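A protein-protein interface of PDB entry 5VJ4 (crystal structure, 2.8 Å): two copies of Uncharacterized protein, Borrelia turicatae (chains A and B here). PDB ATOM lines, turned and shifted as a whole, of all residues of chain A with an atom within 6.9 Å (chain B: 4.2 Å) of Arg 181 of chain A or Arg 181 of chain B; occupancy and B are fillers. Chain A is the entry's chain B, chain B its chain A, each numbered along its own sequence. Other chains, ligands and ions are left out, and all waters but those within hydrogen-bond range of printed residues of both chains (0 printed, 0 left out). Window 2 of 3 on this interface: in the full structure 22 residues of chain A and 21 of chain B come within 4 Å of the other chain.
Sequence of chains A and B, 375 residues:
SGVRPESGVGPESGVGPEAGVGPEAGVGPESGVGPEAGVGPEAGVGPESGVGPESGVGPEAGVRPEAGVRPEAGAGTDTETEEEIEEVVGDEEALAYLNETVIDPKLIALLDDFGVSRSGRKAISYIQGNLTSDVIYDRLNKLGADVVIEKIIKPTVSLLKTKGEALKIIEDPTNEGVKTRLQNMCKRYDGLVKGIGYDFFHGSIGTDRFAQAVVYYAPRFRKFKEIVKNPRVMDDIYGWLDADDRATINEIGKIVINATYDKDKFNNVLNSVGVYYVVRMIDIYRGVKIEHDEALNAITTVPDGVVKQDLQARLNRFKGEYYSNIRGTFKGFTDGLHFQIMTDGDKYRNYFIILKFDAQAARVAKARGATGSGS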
ATOM      1  N   GLU A 176      37.455   0.427  30.029  1.00  0.00           N
ATOM      2  CA  GLU A 176      36.932   1.560  30.773  1.00  0.00           C
ATOM      3  C   GLU A 176      35.807   2.279  30.017  1.00  0.00           C
ATOM      4  O   GLU A 176      34.829   2.703  30.632  1.00  0.00           O
ATOM      5  CB  GLU A 176      38.063   2.529  31.129  1.00  0.00           C
ATOM      6  CG  GLU A 176      37.822   3.316  32.413  1.00  0.00           C
ATOM      7  CD  GLU A 176      36.667   4.307  32.312  1.00  0.00           C
ATOM      8  OE1 GLU A 176      36.552   4.986  31.271  1.00  0.00           O
ATOM      9  OE2 GLU A 176      35.862   4.397  33.265  1.00  0.00           O
ATOM     10  N   GLY A 177      35.954   2.405  28.696  1.00  0.00           N
ATOM     11  CA  GLY A 177      34.941   3.051  27.852  1.00  0.00           C
ATOM     12  C   GLY A 177      33.597   2.365  27.990  1.00  0.00           C
ATOM     13  O   GLY A 177      32.590   2.985  28.331  1.00  0.00           O
ATOM     14  N   VAL A 178      33.602   1.062  27.771  1.00  0.00           N
ATOM     15  CA  VAL A 178      32.407   0.269  27.865  1.00  0.00           C
ATOM     16  C   VAL A 178      32.073  -0.172  29.313  1.00  0.00           C
ATOM     17  O   VAL A 178      31.079  -0.869  29.535  1.00  0.00           O
ATOM     18  CB  VAL A 178      32.515  -0.926  26.908  1.00  0.00           C
ATOM     19  N   LYS A 179      32.870   0.249  30.293  1.00  0.00           N
ATOM     20  CA  LYS A 179      32.736  -0.276  31.659  1.00  0.00           C
ATOM     21  C   LYS A 179      31.326  -0.048  32.217  1.00  0.00           C
ATOM     22  O   LYS A 179      30.616  -1.018  32.507  1.00  0.00           O
ATOM     23  CB  LYS A 179      33.844   0.235  32.617  1.00  0.00           C
ATOM     24  N   THR A 180      30.909   1.214  32.310  1.00  0.00           N
ATOM     25  CA  THR A 180      29.658   1.538  33.003  1.00  0.00           C
ATOM     26  C   THR A 180      28.473   0.826  32.386  1.00  0.00           C
ATOM     27  O   THR A 180      27.711   0.164  33.109  1.00  0.00           O
ATOM     28  CB  THR A 180      29.362   3.035  33.091  1.00  0.00           C
ATOM     29  OG1 THR A 180      30.589   3.769  33.115  1.00  0.00           O
ATOM     30  CG2 THR A 180      28.588   3.298  34.364  1.00  0.00           C
ATOM     31  N   ARG A 181      28.339   0.954  31.062  1.00  0.00           N
ATOM     32  CA  ARG A 181      27.331   0.214  30.294  1.00  0.00           C
ATOM     33  C   ARG A 181      27.265  -1.277  30.675  1.00  0.00           C
ATOM     34  O   ARG A 181      26.191  -1.776  31.035  1.00  0.00           O
ATOM     35  CB  ARG A 181      27.574   0.401  28.809  1.00  0.00           C
ATOM     36  CG  ARG A 181      26.358   0.162  27.930  1.00  0.00           C
ATOM     37  CD  ARG A 181      26.582   0.817  26.577  1.00  0.00           C
ATOM     38  NE  ARG A 181      25.417   0.690  25.713  1.00  0.00           N
ATOM     39  CZ  ARG A 181      25.377   1.070  24.439  1.00  0.00           C
ATOM     40  NH1 ARG A 181      26.443   1.604  23.856  1.00  0.00           N
ATOM     41  NH2 ARG A 181      24.259   0.925  23.746  1.00  0.00           N
ATOM     42  N   LEU A 182      28.413  -1.958  30.675  1.00  0.00           N
ATOM     43  CA  LEU A 182      28.479  -3.369  31.097  1.00  0.00           C
ATOM     44  C   LEU A 182      27.978  -3.608  32.524  1.00  0.00           C
ATOM     45  O   LEU A 182      27.257  -4.569  32.764  1.00  0.00           O
ATOM     46  CB  LEU A 182      29.885  -3.932  30.926  1.00  0.00           C
ATOM     47  CG  LEU A 182      30.430  -4.062  29.502  1.00  0.00           C
ATOM     48  CD1 LEU A 182      31.910  -4.376  29.572  1.00  0.00           C
ATOM     49  CD2 LEU A 182      29.695  -5.119  28.692  1.00  0.00           C
ATOM     50  N   GLN A 183      28.337  -2.728  33.459  1.00  0.00           N
ATOM     51  CA  GLN A 183      27.880  -2.849  34.852  1.00  0.00           C
ATOM     52  C   GLN A 183      26.366  -2.711  34.937  1.00  0.00           C
ATOM     53  O   GLN A 183      25.709  -3.478  35.666  1.00  0.00           O
ATOM     54  CB  GLN A 183      28.546  -1.813  35.763  1.00  0.00           C
ATOM     55  CG  GLN A 183      30.014  -1.582  35.442  1.00  0.00           C
ATOM     56  CD  GLN A 183      30.684  -0.553  36.315  1.00  0.00           C
ATOM     57  OE1 GLN A 183      30.102  -0.076  37.287  1.00  0.00           O
ATOM     58  NE2 GLN A 183      31.928  -0.200  35.969  1.00  0.00           N
ATOM     59  N   ASN A 184      25.822  -1.746  34.182  1.00  0.00           N
ATOM     60  CA  ASN A 184      24.381  -1.526  34.122  1.00  0.00           C
ATOM     61  C   ASN A 184      23.646  -2.775  33.675  1.00  0.00           C
ATOM     62  O   ASN A 184      22.724  -3.249  34.362  1.00  0.00           O
ATOM     63  CB  ASN A 184      24.053  -0.369  33.200  1.00  0.00           C
ATOM     64  CG  ASN A 184      24.341   0.969  33.824  1.00  0.00           C
ATOM     65  OD1 ASN A 184      24.285   1.124  35.049  1.00  0.00           O
ATOM     66  ND2 ASN A 184      24.630   1.960  32.980  1.00  0.00           N
ATOM     67  N   MET A 185      24.080  -3.335  32.550  1.00  0.00           N
ATOM     68  CA  MET A 185      23.477  -4.575  32.087  1.00  0.00           C
ATOM     69  C   MET A 185      23.609  -5.654  33.123  1.00  0.00           C
ATOM     70  O   MET A 185      22.629  -6.363  33.398  1.00  0.00           O
ATOM     71  CB  MET A 185      24.022  -4.982  30.728  1.00  0.00           C
ATOM     72  CG  MET A 185      23.174  -6.113  30.137  1.00  0.00           C
ATOM     73  SD  MET A 185      21.338  -5.569  29.615  1.00  0.00           S
ATOM     74  CE  MET A 185      21.915  -4.354  28.168  1.00  0.00           C
ATOM     75  N   CYS A 186      24.793  -5.760  33.735  1.00  0.00           N
ATOM     76  CA  CYS A 186      24.996  -6.713  34.821  1.00  0.00           C
ATOM     77  C   CYS A 186      23.876  -6.575  35.866  1.00  0.00           C
ATOM     78  O   CYS A 186      23.247  -7.589  36.231  1.00  0.00           O
ATOM     79  CB  CYS A 186      26.393  -6.603  35.441  1.00  0.00           C
ATOM     80  SG  CYS A 186      26.621  -7.582  36.952  1.00  0.00           S
ATOM     81  N   LYS A 187      23.588  -5.335  36.288  1.00  0.00           N
ATOM     82  CA  LYS A 187      22.526  -5.107  37.287  1.00  0.00           C
ATOM     83  C   LYS A 187      21.152  -5.580  36.821  1.00  0.00           C
ATOM     84  O   LYS A 187      20.373  -6.128  37.617  1.00  0.00           O
ATOM     85  CB  LYS A 187      22.444  -3.655  37.739  1.00  0.00           C
ATOM     86  CG  LYS A 187      23.760  -2.981  38.053  1.00  0.00           C
ATOM     87  CD  LYS A 187      23.540  -1.876  39.074  1.00  0.00           C
ATOM     88  CE  LYS A 187      24.448  -0.679  38.808  1.00  0.00           C
ATOM     89  NZ  LYS A 187      24.401   0.315  39.920  1.00  0.00           N
ATOM     90  N   ARG A 188      20.862  -5.395  35.531  1.00  0.00           N
ATOM     91  CA  ARG A 188      19.571  -5.829  34.986  1.00  0.00           C
ATOM     92  C   ARG A 188      19.449  -7.338  35.097  1.00  0.00           C
ATOM     93  O   ARG A 188      18.504  -7.844  35.744  1.00  0.00           O
ATOM     94  CB  ARG A 188      19.398  -5.354  33.555  1.00  0.00           C
ATOM     95  CG  ARG A 188      19.465  -3.847  33.451  1.00  0.00           C
ATOM     96  CD  ARG A 188      19.037  -3.298  32.120  1.00  0.00           C
ATOM     97  NE  ARG A 188      19.249  -1.859  32.115  1.00  0.00           N
ATOM     98  CZ  ARG A 188      20.243  -1.261  31.456  1.00  0.00           C
ATOM     99  NH1 ARG A 188      21.077  -1.993  30.716  1.00  0.00           N
ATOM    100  NH2 ARG A 188      20.392   0.071  31.513  1.00  0.00           N
ATOM    101  N   PHE A 224      29.918 -11.102  27.448  1.00  0.00           N
ATOM    102  CA  PHE A 224      30.682  -9.880  27.709  1.00  0.00           C
ATOM    103  C   PHE A 224      32.053  -9.863  27.026  1.00  0.00           C
ATOM    104  O   PHE A 224      32.378  -8.899  26.310  1.00  0.00           O
ATOM    105  CB  PHE A 224      30.795  -9.655  29.218  1.00  0.00           C
ATOM    106  CG  PHE A 224      29.531  -9.115  29.857  1.00  0.00           C
ATOM    107  CD1 PHE A 224      28.280  -9.266  29.251  1.00  0.00           C
ATOM    108  CD2 PHE A 224      29.587  -8.463  31.088  1.00  0.00           C
ATOM    109  CE1 PHE A 224      27.127  -8.776  29.855  1.00  0.00           C
ATOM    110  CE2 PHE A 224      28.432  -7.970  31.700  1.00  0.00           C
ATOM    111  CZ  PHE A 224      27.208  -8.129  31.082  1.00  0.00           C
ATOM    112  N   PRO A 231      33.278  -3.127  20.351  1.00  0.00           N
ATOM    113  CA  PRO A 231      32.201  -2.480  21.095  1.00  0.00           C
ATOM    114  C   PRO A 231      30.991  -1.963  20.316  1.00  0.00           C
ATOM    115  O   PRO A 231      29.938  -1.839  20.908  1.00  0.00           O
ATOM    116  CB  PRO A 231      32.922  -1.312  21.786  1.00  0.00           C
ATOM    117  CG  PRO A 231      34.276  -1.847  22.047  1.00  0.00           C
ATOM    118  CD  PRO A 231      34.598  -2.649  20.815  1.00  0.00           C
ATOM    119  N   ARG A 232      31.135  -1.657  19.027  1.00  0.00           N
ATOM    120  CA  ARG A 232      30.037  -1.059  18.240  1.00  0.00           C
ATOM    121  C   ARG A 232      28.749  -1.902  18.271  1.00  0.00           C
ATOM    122  O   ARG A 232      27.650  -1.400  18.026  1.00  0.00           O
ATOM    123  CB  ARG A 232      30.472  -0.752  16.785  1.00  0.00           C
ATOM    124  N   VAL A 233      28.906  -3.169  18.630  1.00  0.00           N
ATOM    125  CA  VAL A 233      27.837  -4.157  18.632  1.00  0.00           C
ATOM    126  C   VAL A 233      26.689  -3.869  19.636  1.00  0.00           C
ATOM    127  O   VAL A 233      25.561  -4.288  19.399  1.00  0.00           O
ATOM    128  CB  VAL A 233      28.465  -5.569  18.830  1.00  0.00           C
ATOM    129  CG1 VAL A 233      28.664  -5.917  20.303  1.00  0.00           C
ATOM    130  CG2 VAL A 233      27.665  -6.640  18.108  1.00  0.00           C
ATOM    131  N   MET A 234      26.986  -3.137  20.719  1.00  0.00           N
ATOM    132  CA  MET A 234      26.041  -2.892  21.838  1.00  0.00           C
ATOM    133  C   MET A 234      24.813  -2.066  21.503  1.00  0.00           C
ATOM    134  O   MET A 234      23.764  -2.189  22.130  1.00  0.00           O
ATOM    135  CB  MET A 234      26.761  -2.193  22.977  1.00  0.00           C
ATOM    136  CG  MET A 234      27.699  -3.134  23.727  1.00  0.00           C
ATOM    137  SD  MET A 234      29.045  -2.115  24.755  1.00  0.00           S
ATOM    138  CE  MET A 234      28.491  -2.559  26.581  1.00  0.00           C
ATOM    139  N   ASP A 235      24.909  -1.224  20.499  1.00  0.00           N
ATOM    140  CA  ASP A 235      23.764  -0.418  20.102  1.00  0.00           C
ATOM    141  C   ASP A 235      22.667  -1.243  19.403  1.00  0.00           C
ATOM    142  O   ASP A 235      21.626  -0.716  19.046  1.00  0.00           O
ATOM    143  CB  ASP A 235      24.239   0.735  19.212  1.00  0.00           C
ATOM    144  CG  ASP A 235      25.305   1.601  19.881  1.00  0.00           C
ATOM    145  OD1 ASP A 235      25.190   1.874  21.097  1.00  0.00           O
ATOM    146  OD2 ASP A 235      26.259   2.013  19.194  1.00  0.00           O
ATOM    147  N   ASP A 236      22.916  -2.525  19.185  1.00  0.00           N
ATOM    148  CA  ASP A 236      21.933  -3.423  18.610  1.00  0.00           C
ATOM    149  C   ASP A 236      21.437  -4.356  19.714  1.00  0.00           C
ATOM    150  O   ASP A 236      22.153  -4.640  20.670  1.00  0.00           O
ATOM    151  CB  ASP A 236      22.557  -4.223  17.456  1.00  0.00           C
ATOM    152  CG  ASP A 236      21.521  -4.906  16.564  1.00  0.00           C
ATOM    153  OD1 ASP A 236      20.413  -4.348  16.372  1.00  0.00           O
ATOM    154  OD2 ASP A 236      21.838  -5.994  16.029  1.00  0.00           O
ATOM    155  N   TRP A 240      23.946  -8.382  22.175  1.00  0.00           N
ATOM    156  CA  TRP A 240      24.042  -8.843  23.556  1.00  0.00           C
ATOM    157  C   TRP A 240      23.675 -10.301  23.762  1.00  0.00           C
ATOM    158  O   TRP A 240      23.684 -10.792  24.904  1.00  0.00           O
ATOM    159  CB  TRP A 240      23.131  -7.998  24.434  1.00  0.00           C
ATOM    160  CG  TRP A 240      23.498  -6.562  24.508  1.00  0.00           C
ATOM    161  CD1 TRP A 240      23.174  -5.593  23.609  1.00  0.00           C
ATOM    162  CD2 TRP A 240      24.220  -5.913  25.554  1.00  0.00           C
ATOM    163  NE1 TRP A 240      23.670  -4.375  24.013  1.00  0.00           N
ATOM    164  CE2 TRP A 240      24.314  -4.541  25.208  1.00  0.00           C
ATOM    165  CE3 TRP A 240      24.813  -6.351  26.740  1.00  0.00           C
ATOM    166  CZ2 TRP A 240      24.975  -3.606  26.009  1.00  0.00           C
ATOM    167  CZ3 TRP A 240      25.491  -5.414  27.535  1.00  0.00           C
ATOM    168  CH2 TRP A 240      25.560  -4.062  27.165  1.00  0.00           C
ATOM    169  N   VAL B 178      28.893   7.954  17.941  1.00  0.00           N
ATOM    170  CA  VAL B 178      27.654   7.810  18.725  1.00  0.00           C
ATOM    171  C   VAL B 178      26.374   7.850  17.885  1.00  0.00           C
ATOM    172  O   VAL B 178      25.277   7.677  18.421  1.00  0.00           O
ATOM    173  CB  VAL B 178      27.558   8.854  19.874  1.00  0.00           C
ATOM    174  CG1 VAL B 178      28.648   8.618  20.926  1.00  0.00           C
ATOM    175  CG2 VAL B 178      27.570  10.294  19.343  1.00  0.00           C
ATOM    176  N   LYS B 179      26.513   8.081  16.581  1.00  0.00           N
ATOM    177  CA  LYS B 179      25.377   8.210  15.652  1.00  0.00           C
ATOM    178  C   LYS B 179      24.255   7.197  15.936  1.00  0.00           C
ATOM    179  O   LYS B 179      23.122   7.580  16.255  1.00  0.00           O
ATOM    180  CB  LYS B 179      25.868   8.071  14.201  1.00  0.00           C
ATOM    181  CG  LYS B 179      24.836   8.410  13.138  1.00  0.00           C
ATOM    182  CD  LYS B 179      25.210   7.825  11.783  1.00  0.00           C
ATOM    183  CE  LYS B 179      24.444   8.495  10.648  1.00  0.00           C
ATOM    184  NZ  LYS B 179      24.515   7.649   9.427  1.00  0.00           N
ATOM    185  N   THR B 180      24.609   5.912  15.866  1.00  0.00           N
ATOM    186  CA  THR B 180      23.662   4.823  16.042  1.00  0.00           C
ATOM    187  C   THR B 180      22.834   4.994  17.302  1.00  0.00           C
ATOM    188  O   THR B 180      21.598   4.998  17.240  1.00  0.00           O
ATOM    189  CB  THR B 180      24.367   3.440  16.032  1.00  0.00           C
ATOM    190  OG1 THR B 180      24.850   3.177  14.722  1.00  0.00           O
ATOM    191  CG2 THR B 180      23.414   2.330  16.358  1.00  0.00           C
ATOM    192  N   ARG B 181      23.511   5.169  18.434  1.00  0.00           N
ATOM    193  CA  ARG B 181      22.831   5.152  19.724  1.00  0.00           C
ATOM    194  C   ARG B 181      21.795   6.245  19.831  1.00  0.00           C
ATOM    195  O   ARG B 181      20.753   6.047  20.487  1.00  0.00           O
ATOM    196  CB  ARG B 181      23.816   5.271  20.878  1.00  0.00           C
ATOM    197  CG  ARG B 181      23.364   4.517  22.110  1.00  0.00           C
ATOM    198  CD  ARG B 181      24.477   4.438  23.099  1.00  0.00           C
ATOM    199  NE  ARG B 181      24.001   4.041  24.419  1.00  0.00           N
ATOM    200  CZ  ARG B 181      24.686   4.238  25.543  1.00  0.00           C
ATOM    201  NH1 ARG B 181      25.877   4.839  25.513  1.00  0.00           N
ATOM    202  NH2 ARG B 181      24.190   3.811  26.692  1.00  0.00           N
ATOM    203  N   LEU B 182      22.082   7.385  19.196  1.00  0.00           N
ATOM    204  CA  LEU B 182      21.115   8.466  19.159  1.00  0.00           C
ATOM    205  C   LEU B 182      19.907   8.134  18.288  1.00  0.00           C
ATOM    206  O   LEU B 182      18.768   8.343  18.709  1.00  0.00           O
ATOM    207  CB  LEU B 182      21.771   9.774  18.752  1.00  0.00           C
ATOM    208  CG  LEU B 182      22.802  10.307  19.756  1.00  0.00           C
ATOM    209  CD1 LEU B 182      23.397  11.579  19.198  1.00  0.00           C
ATOM    210  CD2 LEU B 182      22.228  10.580  21.147  1.00  0.00           C
ATOM    211  N   GLN B 183      20.156   7.585  17.099  1.00  0.00           N
ATOM    212  CA  GLN B 183      19.075   7.170  16.216  1.00  0.00           C
ATOM    213  C   GLN B 183      18.128   6.212  16.951  1.00  0.00           C
ATOM    214  O   GLN B 183      16.907   6.416  16.910  1.00  0.00           O
ATOM    215  CB  GLN B 183      19.618   6.517  14.962  1.00  0.00           C
ATOM    216  CG  GLN B 183      20.296   7.483  14.013  1.00  0.00           C
ATOM    217  CD  GLN B 183      20.987   6.777  12.864  1.00  0.00           C
ATOM    218  OE1 GLN B 183      21.463   5.645  13.007  1.00  0.00           O
ATOM    219  NE2 GLN B 183      21.062   7.449  11.719  1.00  0.00           N
ATOM    220  N   ASN B 184      18.678   5.208  17.650  1.00  0.00           N
ATOM    221  CA  ASN B 184      17.833   4.295  18.406  1.00  0.00           C
ATOM    222  C   ASN B 184      16.936   5.007  19.403  1.00  0.00           C
ATOM    223  O   ASN B 184      15.736   4.732  19.467  1.00  0.00           O
ATOM    224  CB  ASN B 184      18.658   3.214  19.072  1.00  0.00           C
ATOM    225  CG  ASN B 184      19.429   2.397  18.062  1.00  0.00           C
ATOM    226  OD1 ASN B 184      19.365   2.660  16.863  1.00  0.00           O
ATOM    227  ND2 ASN B 184      20.151   1.395  18.535  1.00  0.00           N
ATOM    228  N   MET B 185      17.506   5.954  20.144  1.00  0.00           N
ATOM    229  CA  MET B 185      16.687   6.728  21.040  1.00  0.00           C
ATOM    230  C   MET B 185      15.684   7.506  20.218  1.00  0.00           C
ATOM    231  O   MET B 185      14.488   7.516  20.540  1.00  0.00           O
ATOM    232  CB  MET B 185      17.497   7.624  21.947  1.00  0.00           C
ATOM    233  CG  MET B 185      16.688   8.059  23.184  1.00  0.00           C
ATOM    234  SD  MET B 185      16.036   6.567  24.321  1.00  0.00           S
ATOM    235  CE  MET B 185      17.806   6.019  25.021  1.00  0.00           C
ATOM    236  N   MET B 234      25.140   9.293  28.466  1.00  0.00           N
ATOM    237  CA  MET B 234      24.233   8.234  27.966  1.00  0.00           C
ATOM    238  C   MET B 234      24.179   6.979  28.811  1.00  0.00           C
ATOM    239  O   MET B 234      23.164   6.282  28.803  1.00  0.00           O
ATOM    240  CB  MET B 234      24.543   7.815  26.537  1.00  0.00           C
ATOM    241  CG  MET B 234      24.862   9.030  25.690  1.00  0.00           C
ATOM    242  SD  MET B 234      24.895   8.498  23.791  1.00  0.00           S
ATOM    243  CE  MET B 234      26.171   9.876  23.201  1.00  0.00           C
ATOM    244  N   ASP B 235      25.235   6.676  29.558  1.00  0.00           N
ATOM    245  CA  ASP B 235      25.223   5.481  30.401  1.00  0.00           C
ATOM    246  C   ASP B 235      24.379   5.666  31.678  1.00  0.00           C
ATOM    247  O   ASP B 235      24.310   4.767  32.515  1.00  0.00           O
ATOM    248  CB  ASP B 235      26.650   5.036  30.748  1.00  0.00           C
ATOM    249  CG  ASP B 235      27.435   4.541  29.532  1.00  0.00           C
ATOM    250  OD1 ASP B 235      26.805   4.076  28.554  1.00  0.00           O
ATOM    251  OD2 ASP B 235      28.690   4.613  29.569  1.00  0.00           O
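O of Asp 235 of chain A lies within hydrogen-bond range of ND2 of Asn 184 of chain B, 2.6 Å away. The backbone carbonyl oxygen (O) of Asp 235 of chain B lies within hydrogen-bond range of the side-chain amide nitrogen (ND2) of Asn 184 of chain A, at 2.9 Å. The guanidinium group (NE) of Arg 181 of chain B lies close to the guanidinium group (NH2) of Arg 181 of chain A, 3.2 Å away.
Thr 180 of chain A touches Asp 235 of chain B, and with the chains exchanged Asp 235 of chain A touches Thr 180 of chain B. Arg 181 of chain B touches its own counterpart, Arg 181 of chain A. Arg 181 of chain A touches Asp 235 of chain B, and with the chains exchanged Asp 235 of chain A touches Arg 181 of chain B. Asn 184 of chain A touches Asp 235 of chain B, and with the chains exchanged Asp 235 of chain A touches Asn 184 of chain B. Positions printed for both chains: 178, 179, 180, 181, 182, 183, 184, 185, 234 and 235.
Thr 180 of chain A touches Asp 235 of chain B. CB of Arg 181 of chain A touches OD1 of Asp 235 of chain B (3.8 Å). Asp 235 of chain A touches Thr 180 of chain B. Asp 235 of chain A touches Arg 181 of chain B (OD1 to CD, 3.3 Å).
Of the 10 printed residues of chain B, 4 touch a printed residue of chain A. Printed residues of chain A that touch a printed residue of chain B: Thr 180, Arg 181, Asn 184 and Asp 235. Among the printed residues, 7 pairs touch across the chains. Among the printed residues, no Asp or Glu carboxylate lies within 4 Å of a Lys or Arg side-chain nitrogen of the other chain.
OD1 of Asn 184 of chain B sits close to O of Thr 180 of chain B (3.3 Å). The guanidinium group of Arg 181 of chain B lies within hydrogen-bond range of the backbone carbonyl oxygen of Met 234 of chain B (3.4 Å). The side-chain carboxylate of Asp 235 of chain B lies within salt-bridge range of the guanidinium group of Arg 181 of chain B, at 3.2 Å. The guanidinium group (NH2) of Arg 181 of chain A lies within salt-bridge range of the side-chain carboxylate (OD1) of Asp 235 of chain A, 3.0 Å away.
Of chain B, only Arg 181 and Asp 235 come within 4 Å of Arg 181 of chain A. Of the printed residues of chain A, Thr 180 of chain B touches Asp 235. Of the printed residues of chain B, Thr 180 of chain A touches Asp 235. Of the printed residues of chain B, Asp 235 of chain A touches Thr 180 (3.4 Å), Arg 181 (3.3 Å) and Asn 184 (2.6 Å). Printed residues of chain A within 4 Å of Asn 184 of chain B: Asp 235 (2.6 Å). The nearest printed residue of chain B that does not touch Arg 181 of chain A is Asn 184 of chain B (6.7 Å).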
